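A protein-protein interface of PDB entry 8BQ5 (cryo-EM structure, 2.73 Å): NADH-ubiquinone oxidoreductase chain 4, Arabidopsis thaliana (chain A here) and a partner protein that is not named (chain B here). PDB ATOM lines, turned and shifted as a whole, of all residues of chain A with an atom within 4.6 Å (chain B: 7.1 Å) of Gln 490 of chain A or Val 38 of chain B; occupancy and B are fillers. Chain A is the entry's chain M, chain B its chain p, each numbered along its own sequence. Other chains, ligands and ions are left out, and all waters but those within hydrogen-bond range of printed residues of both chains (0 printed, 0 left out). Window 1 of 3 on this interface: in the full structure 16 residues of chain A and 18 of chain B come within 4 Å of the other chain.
OE1 of Glu 35 of chain B lies within salt-bridge range of NH1 of Arg 39 of chain B (3.98 Å).
The guanidinium group (NE) of Arg 34 of chain B lies close to the side-chain amide nitrogen (ND2) of Asn 487 of chain A.
A ring nitrogen (ND1) of His 491 of chain A is in hydrogen-bond range of the guanidinium group (NH1) of Arg 34 of chain B.
The backbone carbonyl oxygen of His 495 of chain A lies within hydrogen-bond range of the side-chain amino group of Lys 41 of chain B, 3.5 Å away.
The side-chain amide oxygen (OE1) of Gln 490 of chain A lies close to the side-chain amino group (NZ) of Lys 41 of chain B (3.5 Å).
OG of Ser 486 of chain A sits at hydrogen-bond distance from NE1 of Trp 42 of chain B, 2.7 Å away.
Val 38 of chain B touches Ser 486 of chain A.
CG of Glu 35 of chain B touches ND2 of Asn 487 of chain A (3.9 Å).
OD1 of Asn 487 of chain A touches CG2 of Val 38 of chain B, at 3.8 Å.
CG1 of Val 489 of chain A touches CD1 of Trp 86 of chain B, 3.3 Å away.
Ile 37 of chain B touches Gln 490 of chain A.
Val 38 of chain B touches Gln 490 of chain A (CG2 to CB, 3.6 Å).
Gln 490 of chain A touches Trp 86 of chain B.
Printed residues of chain A that touch a printed residue of chain B: Ser 486, Asn 487, Val 489, Gln 490, His 491 and His 495.
Hydrophobic or aromatic side chains of chain A that line the printed part of chain B: Val 489 and His 491.
Printed residues of chain B that touch a printed residue of chain A: Arg 34, Glu 35, Ile 37, Val 38, Lys 41, Trp 42 and Trp 86.
Hydrophobic or aromatic side chains of chain B that line the printed part of chain A: Ile 37, Val 38, Trp 42 and Trp 86.
Among the printed residues, 12 pairs touch across the chains.
Of chain A, only Ser 486, Asn 487 and Gln 490 come within 4 Å of Val 38 of chain B.
Of the printed residues of chain B, Asn 487 of chain A touches Arg 34 (2.8 Å), Glu 35 (3.9 Å) and Val 38 (3.8 Å).
Printed residues of chain B within 4 Å of His 491 of chain A: Arg 34.
Printed residues of chain B within 4 Å of Ser 486 of chain A: Val 38 and Trp 42.
Of the printed residues of chain B, Val 489 of chain A touches Trp 86 (3.3 Å).
The nearest residue of chain B that does not touch Gln 490 of chain A is Arg 34 of chain B (4.1 Å).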
ATOM      1  N   SER A 486      28.418 -20.019 -29.232  1.00  0.00           N
ATOM      2  CA  SER A 486      28.378 -20.510 -27.859  1.00  0.00           C
ATOM      3  C   SER A 486      29.772 -20.848 -27.354  1.00  0.00           C
ATOM      4  O   SER A 486      30.127 -20.519 -26.216  1.00  0.00           O
ATOM      5  CB  SER A 486      27.477 -21.740 -27.768  1.00  0.00           C
ATOM      6  OG  SER A 486      26.113 -21.379 -27.828  1.00  0.00           O
ATOM      7  N   ASN A 487      30.575 -21.512 -28.186  1.00  0.00           N
ATOM      8  CA  ASN A 487      31.921 -21.890 -27.779  1.00  0.00           C
ATOM      9  C   ASN A 487      32.839 -20.680 -27.691  1.00  0.00           C
ATOM     10  O   ASN A 487      33.830 -20.707 -26.954  1.00  0.00           O
ATOM     11  CB  ASN A 487      32.486 -22.922 -28.750  1.00  0.00           C
ATOM     12  CG  ASN A 487      32.237 -24.339 -28.292  1.00  0.00           C
ATOM     13  OD1 ASN A 487      31.184 -24.910 -28.557  1.00  0.00           O
ATOM     14  ND2 ASN A 487      33.204 -24.915 -27.598  1.00  0.00           N
ATOM     15  N   LEU A 488      32.517 -19.616 -28.429  1.00  0.00           N
ATOM     16  CA  LEU A 488      33.314 -18.366 -28.323  1.00  0.00           C
ATOM     17  C   LEU A 488      33.042 -17.733 -26.954  1.00  0.00           C
ATOM     18  O   LEU A 488      34.011 -17.284 -26.310  1.00  0.00           O
ATOM     19  CB  LEU A 488      32.914 -17.432 -29.469  1.00  0.00           C
ATOM     20  CG  LEU A 488      33.463 -16.009 -29.410  1.00  0.00           C
ATOM     21  CD1 LEU A 488      34.980 -16.010 -29.488  1.00  0.00           C
ATOM     22  CD2 LEU A 488      32.880 -15.169 -30.532  1.00  0.00           C
ATOM     23  N   VAL A 489      31.779 -17.728 -26.516  1.00  0.00           N
ATOM     24  CA  VAL A 489      31.435 -17.099 -25.246  1.00  0.00           C
ATOM     25  C   VAL A 489      31.977 -17.915 -24.077  1.00  0.00           C
ATOM     26  O   VAL A 489      32.457 -17.358 -23.082  1.00  0.00           O
ATOM     27  CB  VAL A 489      29.910 -16.907 -25.157  1.00  0.00           C
ATOM     28  CG1 VAL A 489      29.496 -16.571 -23.745  1.00  0.00           C
ATOM     29  CG2 VAL A 489      29.453 -15.821 -26.120  1.00  0.00           C
ATOM     30  N   GLN A 490      31.920 -19.243 -24.181  1.00  0.00           N
ATOM     31  CA  GLN A 490      32.344 -20.114 -23.092  1.00  0.00           C
ATOM     32  C   GLN A 490      33.858 -20.224 -22.968  1.00  0.00           C
ATOM     33  O   GLN A 490      34.351 -20.662 -21.924  1.00  0.00           O
ATOM     34  CB  GLN A 490      31.744 -21.508 -23.281  1.00  0.00           C
ATOM     35  CG  GLN A 490      31.970 -22.440 -22.113  1.00  0.00           C
ATOM     36  CD  GLN A 490      31.072 -22.100 -20.950  1.00  0.00           C
ATOM     37  OE1 GLN A 490      29.889 -22.427 -20.953  1.00  0.00           O
ATOM     38  NE2 GLN A 490      31.628 -21.428 -19.948  1.00  0.00           N
ATOM     39  N   HIS A 491      34.574 -19.794 -24.010  1.00  0.00           N
ATOM     40  CA  HIS A 491      36.056 -19.923 -24.031  1.00  0.00           C
ATOM     41  C   HIS A 491      36.706 -19.258 -22.819  1.00  0.00           C
ATOM     42  O   HIS A 491      36.410 -18.084 -22.549  1.00  0.00           O
ATOM     43  CB  HIS A 491      36.623 -19.346 -25.334  1.00  0.00           C
ATOM     44  CG  HIS A 491      38.007 -19.811 -25.635  1.00  0.00           C
ATOM     45  ND1 HIS A 491      38.268 -20.793 -26.565  1.00  0.00           N
ATOM     46  CD2 HIS A 491      39.204 -19.442 -25.132  1.00  0.00           C
ATOM     47  CE1 HIS A 491      39.565 -21.010 -26.621  1.00  0.00           C
ATOM     48  NE2 HIS A 491      40.162 -20.191 -25.755  1.00  0.00           N
ATOM     49  N   GLY A 492      37.555 -19.995 -22.108  1.00  0.00           N
ATOM     50  CA  GLY A 492      38.314 -19.410 -21.024  1.00  0.00           C
ATOM     51  C   GLY A 492      37.755 -19.651 -19.638  1.00  0.00           C
ATOM     52  O   GLY A 492      38.454 -19.376 -18.656  1.00  0.00           O
ATOM     53  N   LYS A 493      36.523 -20.144 -19.527  1.00  0.00           N
ATOM     54  CA  LYS A 493      35.908 -20.462 -18.246  1.00  0.00           C
ATOM     55  C   LYS A 493      35.401 -21.897 -18.278  1.00  0.00           C
ATOM     56  O   LYS A 493      35.203 -22.475 -19.350  1.00  0.00           O
ATOM     57  CB  LYS A 493      34.756 -19.501 -17.916  1.00  0.00           C
ATOM     58  CG  LYS A 493      34.092 -18.888 -19.136  1.00  0.00           C
ATOM     59  CD  LYS A 493      32.890 -18.038 -18.753  1.00  0.00           C
ATOM     60  CE  LYS A 493      33.261 -16.950 -17.760  1.00  0.00           C
ATOM     61  NZ  LYS A 493      32.375 -15.760 -17.893  1.00  0.00           N
ATOM     62  N   HIS A 495      32.719 -23.204 -15.965  1.00  0.00           N
ATOM     63  CA  HIS A 495      31.567 -23.365 -15.086  1.00  0.00           C
ATOM     64  C   HIS A 495      30.342 -22.667 -15.665  1.00  0.00           C
ATOM     65  O   HIS A 495      30.449 -21.889 -16.611  1.00  0.00           O
ATOM     66  CB  HIS A 495      31.876 -22.830 -13.687  1.00  0.00           C
ATOM     67  CG  HIS A 495      32.138 -21.357 -13.646  1.00  0.00           C
ATOM     68  ND1 HIS A 495      31.147 -20.417 -13.834  1.00  0.00           N
ATOM     69  CD2 HIS A 495      33.282 -20.662 -13.441  1.00  0.00           C
ATOM     70  CE1 HIS A 495      31.671 -19.207 -13.747  1.00  0.00           C
ATOM     71  NE2 HIS A 495      32.964 -19.328 -13.508  1.00  0.00           N
ATOM     72  N   MET B  33      36.264 -30.471 -22.898  1.00  0.00           N
ATOM     73  CA  MET B  33      35.524 -30.015 -21.723  1.00  0.00           C
ATOM     74  C   MET B  33      34.719 -28.757 -22.025  1.00  0.00           C
ATOM     75  O   MET B  33      33.567 -28.633 -21.591  1.00  0.00           O
ATOM     76  CB  MET B  33      36.485 -29.770 -20.561  1.00  0.00           C
ATOM     77  CG  MET B  33      35.832 -29.266 -19.280  1.00  0.00           C
ATOM     78  SD  MET B  33      34.739 -30.439 -18.458  1.00  0.00           S
ATOM     79  CE  MET B  33      34.195 -29.444 -17.072  1.00  0.00           C
ATOM     80  N   ARG B  34      35.310 -27.811 -22.758  1.00  0.00           N
ATOM     81  CA  ARG B  34      34.586 -26.603 -23.143  1.00  0.00           C
ATOM     82  C   ARG B  34      33.370 -26.947 -23.990  1.00  0.00           C
ATOM     83  O   ARG B  34      32.287 -26.379 -23.810  1.00  0.00           O
ATOM     84  CB  ARG B  34      35.518 -25.652 -23.899  1.00  0.00           C
ATOM     85  CG  ARG B  34      34.892 -24.309 -24.243  1.00  0.00           C
ATOM     86  CD  ARG B  34      35.729 -23.547 -25.257  1.00  0.00           C
ATOM     87  NE  ARG B  34      35.653 -24.145 -26.582  1.00  0.00           N
ATOM     88  CZ  ARG B  34      36.689 -24.318 -27.391  1.00  0.00           C
ATOM     89  NH1 ARG B  34      37.905 -23.932 -27.045  1.00  0.00           N
ATOM     90  NH2 ARG B  34      36.498 -24.888 -28.577  1.00  0.00           N
ATOM     91  N   GLU B  35      33.545 -27.884 -24.918  1.00  0.00           N
ATOM     92  CA  GLU B  35      32.420 -28.332 -25.773  1.00  0.00           C
ATOM     93  C   GLU B  35      31.341 -28.986 -24.913  1.00  0.00           C
ATOM     94  O   GLU B  35      30.154 -28.714 -25.168  1.00  0.00           O
ATOM     95  CB  GLU B  35      32.934 -29.340 -26.793  1.00  0.00           C
ATOM     96  CG  GLU B  35      33.879 -28.735 -27.805  1.00  0.00           C
ATOM     97  CD  GLU B  35      34.444 -29.757 -28.773  1.00  0.00           C
ATOM     98  OE1 GLU B  35      34.247 -30.960 -28.537  1.00  0.00           O
ATOM     99  OE2 GLU B  35      35.060 -29.340 -29.770  1.00  0.00           O
ATOM    100  N   HIS B  36      31.736 -29.827 -23.950  1.00  0.00           N
ATOM    101  CA  HIS B  36      30.765 -30.480 -23.076  1.00  0.00           C
ATOM    102  C   HIS B  36      29.958 -29.463 -22.281  1.00  0.00           C
ATOM    103  O   HIS B  36      28.735 -29.597 -22.149  1.00  0.00           O
ATOM    104  CB  HIS B  36      31.476 -31.445 -22.126  1.00  0.00           C
ATOM    105  CG  HIS B  36      30.544 -32.261 -21.285  1.00  0.00           C
ATOM    106  ND1 HIS B  36      29.725 -33.237 -21.809  1.00  0.00           N
ATOM    107  CD2 HIS B  36      30.290 -32.233 -19.954  1.00  0.00           C
ATOM    108  CE1 HIS B  36      29.015 -33.783 -20.839  1.00  0.00           C
ATOM    109  NE2 HIS B  36      29.338 -33.191 -19.704  1.00  0.00           N
ATOM    110  N   ILE B  37      30.623 -28.438 -21.748  1.00  0.00           N
ATOM    111  CA  ILE B  37      29.931 -27.436 -20.943  1.00  0.00           C
ATOM    112  C   ILE B  37      28.907 -26.688 -21.788  1.00  0.00           C
ATOM    113  O   ILE B  37      27.796 -26.396 -21.331  1.00  0.00           O
ATOM    114  CB  ILE B  37      30.947 -26.479 -20.293  1.00  0.00           C
ATOM    115  CG1 ILE B  37      31.699 -27.190 -19.169  1.00  0.00           C
ATOM    116  CG2 ILE B  37      30.253 -25.269 -19.720  1.00  0.00           C
ATOM    117  CD1 ILE B  37      32.944 -26.465 -18.727  1.00  0.00           C
ATOM    118  N   VAL B  38      29.263 -26.370 -23.036  1.00  0.00           N
ATOM    119  CA  VAL B  38      28.330 -25.676 -23.920  1.00  0.00           C
ATOM    120  C   VAL B  38      27.096 -26.532 -24.167  1.00  0.00           C
ATOM    121  O   VAL B  38      25.959 -26.047 -24.092  1.00  0.00           O
ATOM    122  CB  VAL B  38      29.031 -25.297 -25.239  1.00  0.00           C
ATOM    123  CG1 VAL B  38      28.019 -25.154 -26.362  1.00  0.00           C
ATOM    124  CG2 VAL B  38      29.829 -24.021 -25.069  1.00  0.00           C
ATOM    125  N   ARG B  39      27.298 -27.821 -24.451  1.00  0.00           N
ATOM    126  CA  ARG B  39      26.173 -28.713 -24.705  1.00  0.00           C
ATOM    127  C   ARG B  39      25.302 -28.865 -23.465  1.00  0.00           C
ATOM    128  O   ARG B  39      24.071 -28.932 -23.566  1.00  0.00           O
ATOM    129  CB  ARG B  39      26.683 -30.073 -25.177  1.00  0.00           C
ATOM    130  CG  ARG B  39      26.432 -30.360 -26.648  1.00  0.00           C
ATOM    131  CD  ARG B  39      27.700 -30.786 -27.354  1.00  0.00           C
ATOM    132  NE  ARG B  39      28.455 -31.765 -26.585  1.00  0.00           N
ATOM    133  CZ  ARG B  39      29.709 -32.108 -26.844  1.00  0.00           C
ATOM    134  NH1 ARG B  39      30.375 -31.578 -27.855  1.00  0.00           N
ATOM    135  NH2 ARG B  39      30.310 -33.006 -26.067  1.00  0.00           N
ATOM    136  N   GLU B  40      25.923 -28.930 -22.286  1.00  0.00           N
ATOM    137  CA  GLU B  40      25.155 -29.033 -21.051  1.00  0.00           C
ATOM    138  C   GLU B  40      24.315 -27.784 -20.829  1.00  0.00           C
ATOM    139  O   GLU B  40      23.150 -27.870 -20.427  1.00  0.00           O
ATOM    140  CB  GLU B  40      26.085 -29.276 -19.855  1.00  0.00           C
ATOM    141  CG  GLU B  40      26.661 -30.708 -19.670  1.00  0.00           C
ATOM    142  CD  GLU B  40      25.625 -31.839 -19.659  1.00  0.00           C
ATOM    143  OE1 GLU B  40      24.575 -31.733 -20.321  1.00  0.00           O
ATOM    144  OE2 GLU B  40      25.862 -32.858 -18.981  1.00  0.00           O
ATOM    145  N   LYS B  41      24.893 -26.608 -21.084  1.00  0.00           N
ATOM    146  CA  LYS B  41      24.151 -25.366 -20.894  1.00  0.00           C
ATOM    147  C   LYS B  41      22.990 -25.261 -21.871  1.00  0.00           C
ATOM    148  O   LYS B  41      21.937 -24.706 -21.537  1.00  0.00           O
ATOM    149  CB  LYS B  41      25.085 -24.166 -21.040  1.00  0.00           C
ATOM    150  CG  LYS B  41      25.952 -23.907 -19.822  1.00  0.00           C
ATOM    151  CD  LYS B  41      26.763 -22.637 -19.994  1.00  0.00           C
ATOM    152  CE  LYS B  41      27.509 -22.274 -18.725  1.00  0.00           C
ATOM    153  NZ  LYS B  41      27.837 -20.824 -18.682  1.00  0.00           N
ATOM    154  N   TRP B  42      23.160 -25.786 -23.085  1.00  0.00           N
ATOM    155  CA  TRP B  42      22.079 -25.730 -24.061  1.00  0.00           C
ATOM    156  C   TRP B  42      20.925 -26.633 -23.651  1.00  0.00           C
ATOM    157  O   TRP B  42      19.762 -26.335 -23.940  1.00  0.00           O
ATOM    158  CB  TRP B  42      22.601 -26.104 -25.446  1.00  0.00           C
ATOM    159  CG  TRP B  42      23.115 -24.924 -26.205  1.00  0.00           C
ATOM    160  CD1 TRP B  42      24.420 -24.615 -26.453  1.00  0.00           C
ATOM    161  CD2 TRP B  42      22.336 -23.877 -26.792  1.00  0.00           C
ATOM    162  NE1 TRP B  42      24.501 -23.447 -27.170  1.00  0.00           N
ATOM    163  CE2 TRP B  42      23.235 -22.974 -27.392  1.00  0.00           C
ATOM    164  CE3 TRP B  42      20.964 -23.618 -26.876  1.00  0.00           C
ATOM    165  CZ2 TRP B  42      22.808 -21.831 -28.064  1.00  0.00           C
ATOM    166  CZ3 TRP B  42      20.542 -22.484 -27.544  1.00  0.00           C
ATOM    167  CH2 TRP B  42      21.462 -21.604 -28.130  1.00  0.00           C
ATOM    168  N   ILE B  43      21.229 -27.742 -22.974  1.00  0.00           N
ATOM    169  CA  ILE B  43      20.178 -28.600 -22.439  1.00  0.00           C
ATOM    170  C   ILE B  43      19.374 -27.857 -21.377  1.00  0.00           C
ATOM    171  O   ILE B  43      18.141 -27.944 -21.340  1.00  0.00           O
ATOM    172  CB  ILE B  43      20.784 -29.909 -21.897  1.00  0.00           C
ATOM    173  CG1 ILE B  43      21.362 -30.737 -23.046  1.00  0.00           C
ATOM    174  CG2 ILE B  43      19.744 -30.717 -21.142  1.00  0.00           C
ATOM    175  CD1 ILE B  43      22.392 -31.747 -22.611  1.00  0.00           C
ATOM    176  N   GLN B  44      20.055 -27.108 -20.502  1.00  0.00           N
ATOM    177  CA  GLN B  44      19.341 -26.315 -19.504  1.00  0.00           C
ATOM    178  C   GLN B  44      18.485 -25.237 -20.155  1.00  0.00           C
ATOM    179  O   GLN B  44      17.362 -24.976 -19.708  1.00  0.00           O
ATOM    180  CB  GLN B  44      20.315 -25.676 -18.512  1.00  0.00           C
ATOM    181  CG  GLN B  44      21.583 -26.457 -18.263  1.00  0.00           C
ATOM    182  CD  GLN B  44      21.391 -27.580 -17.265  1.00  0.00           C
ATOM    183  OE1 GLN B  44      20.387 -28.291 -17.297  1.00  0.00           O
ATOM    184  NE2 GLN B  44      22.361 -27.753 -16.377  1.00  0.00           N
ATOM    185  N   ILE B  45      19.004 -24.581 -21.196  1.00  0.00           N
ATOM    186  CA  ILE B  45      18.229 -23.545 -21.874  1.00  0.00           C
ATOM    187  C   ILE B  45      16.960 -24.140 -22.466  1.00  0.00           C
ATOM    188  O   ILE B  45      15.869 -23.570 -22.346  1.00  0.00           O
ATOM    189  CB  ILE B  45      19.071 -22.843 -22.954  1.00  0.00           C
ATOM    190  CG1 ILE B  45      20.245 -22.090 -22.335  1.00  0.00           C
ATOM    191  CG2 ILE B  45      18.211 -21.886 -23.760  1.00  0.00           C
ATOM    192  CD1 ILE B  45      21.456 -22.067 -23.220  1.00  0.00           C
ATOM    193  N   GLY B  85      21.754 -20.279 -19.397  1.00  0.00           N
ATOM    194  CA  GLY B  85      22.432 -19.685 -20.529  1.00  0.00           C
ATOM    195  C   GLY B  85      23.611 -18.821 -20.137  1.00  0.00           C
ATOM    196  O   GLY B  85      24.433 -19.209 -19.302  1.00  0.00           O
ATOM    197  N   TRP B  86      23.688 -17.631 -20.724  1.00  0.00           N
ATOM    198  CA  TRP B  86      24.814 -16.729 -20.530  1.00  0.00           C
ATOM    199  C   TRP B  86      24.339 -15.323 -20.172  1.00  0.00           C
ATOM    200  O   TRP B  86      25.015 -14.335 -20.465  1.00  0.00           O
ATOM    201  CB  TRP B  86      25.695 -16.716 -21.777  1.00  0.00           C
ATOM    202  CG  TRP B  86      26.433 -18.012 -22.001  1.00  0.00           C
ATOM    203  CD1 TRP B  86      27.699 -18.308 -21.601  1.00  0.00           C
ATOM    204  CD2 TRP B  86      25.941 -19.182 -22.669  1.00  0.00           C
ATOM    205  NE1 TRP B  86      28.034 -19.583 -21.984  1.00  0.00           N
ATOM    206  CE2 TRP B  86      26.970 -20.143 -22.639  1.00  0.00           C
ATOM    207  CE3 TRP B  86      24.733 -19.511 -23.288  1.00  0.00           C
ATOM    208  CZ2 TRP B  86      26.830 -21.407 -23.208  1.00  0.00           C
ATOM    209  CZ3 TRP B  86      24.597 -20.767 -23.852  1.00  0.00           C
ATOM    210  CH2 TRP B  86      25.637 -21.699 -23.804  1.00  0.00           C
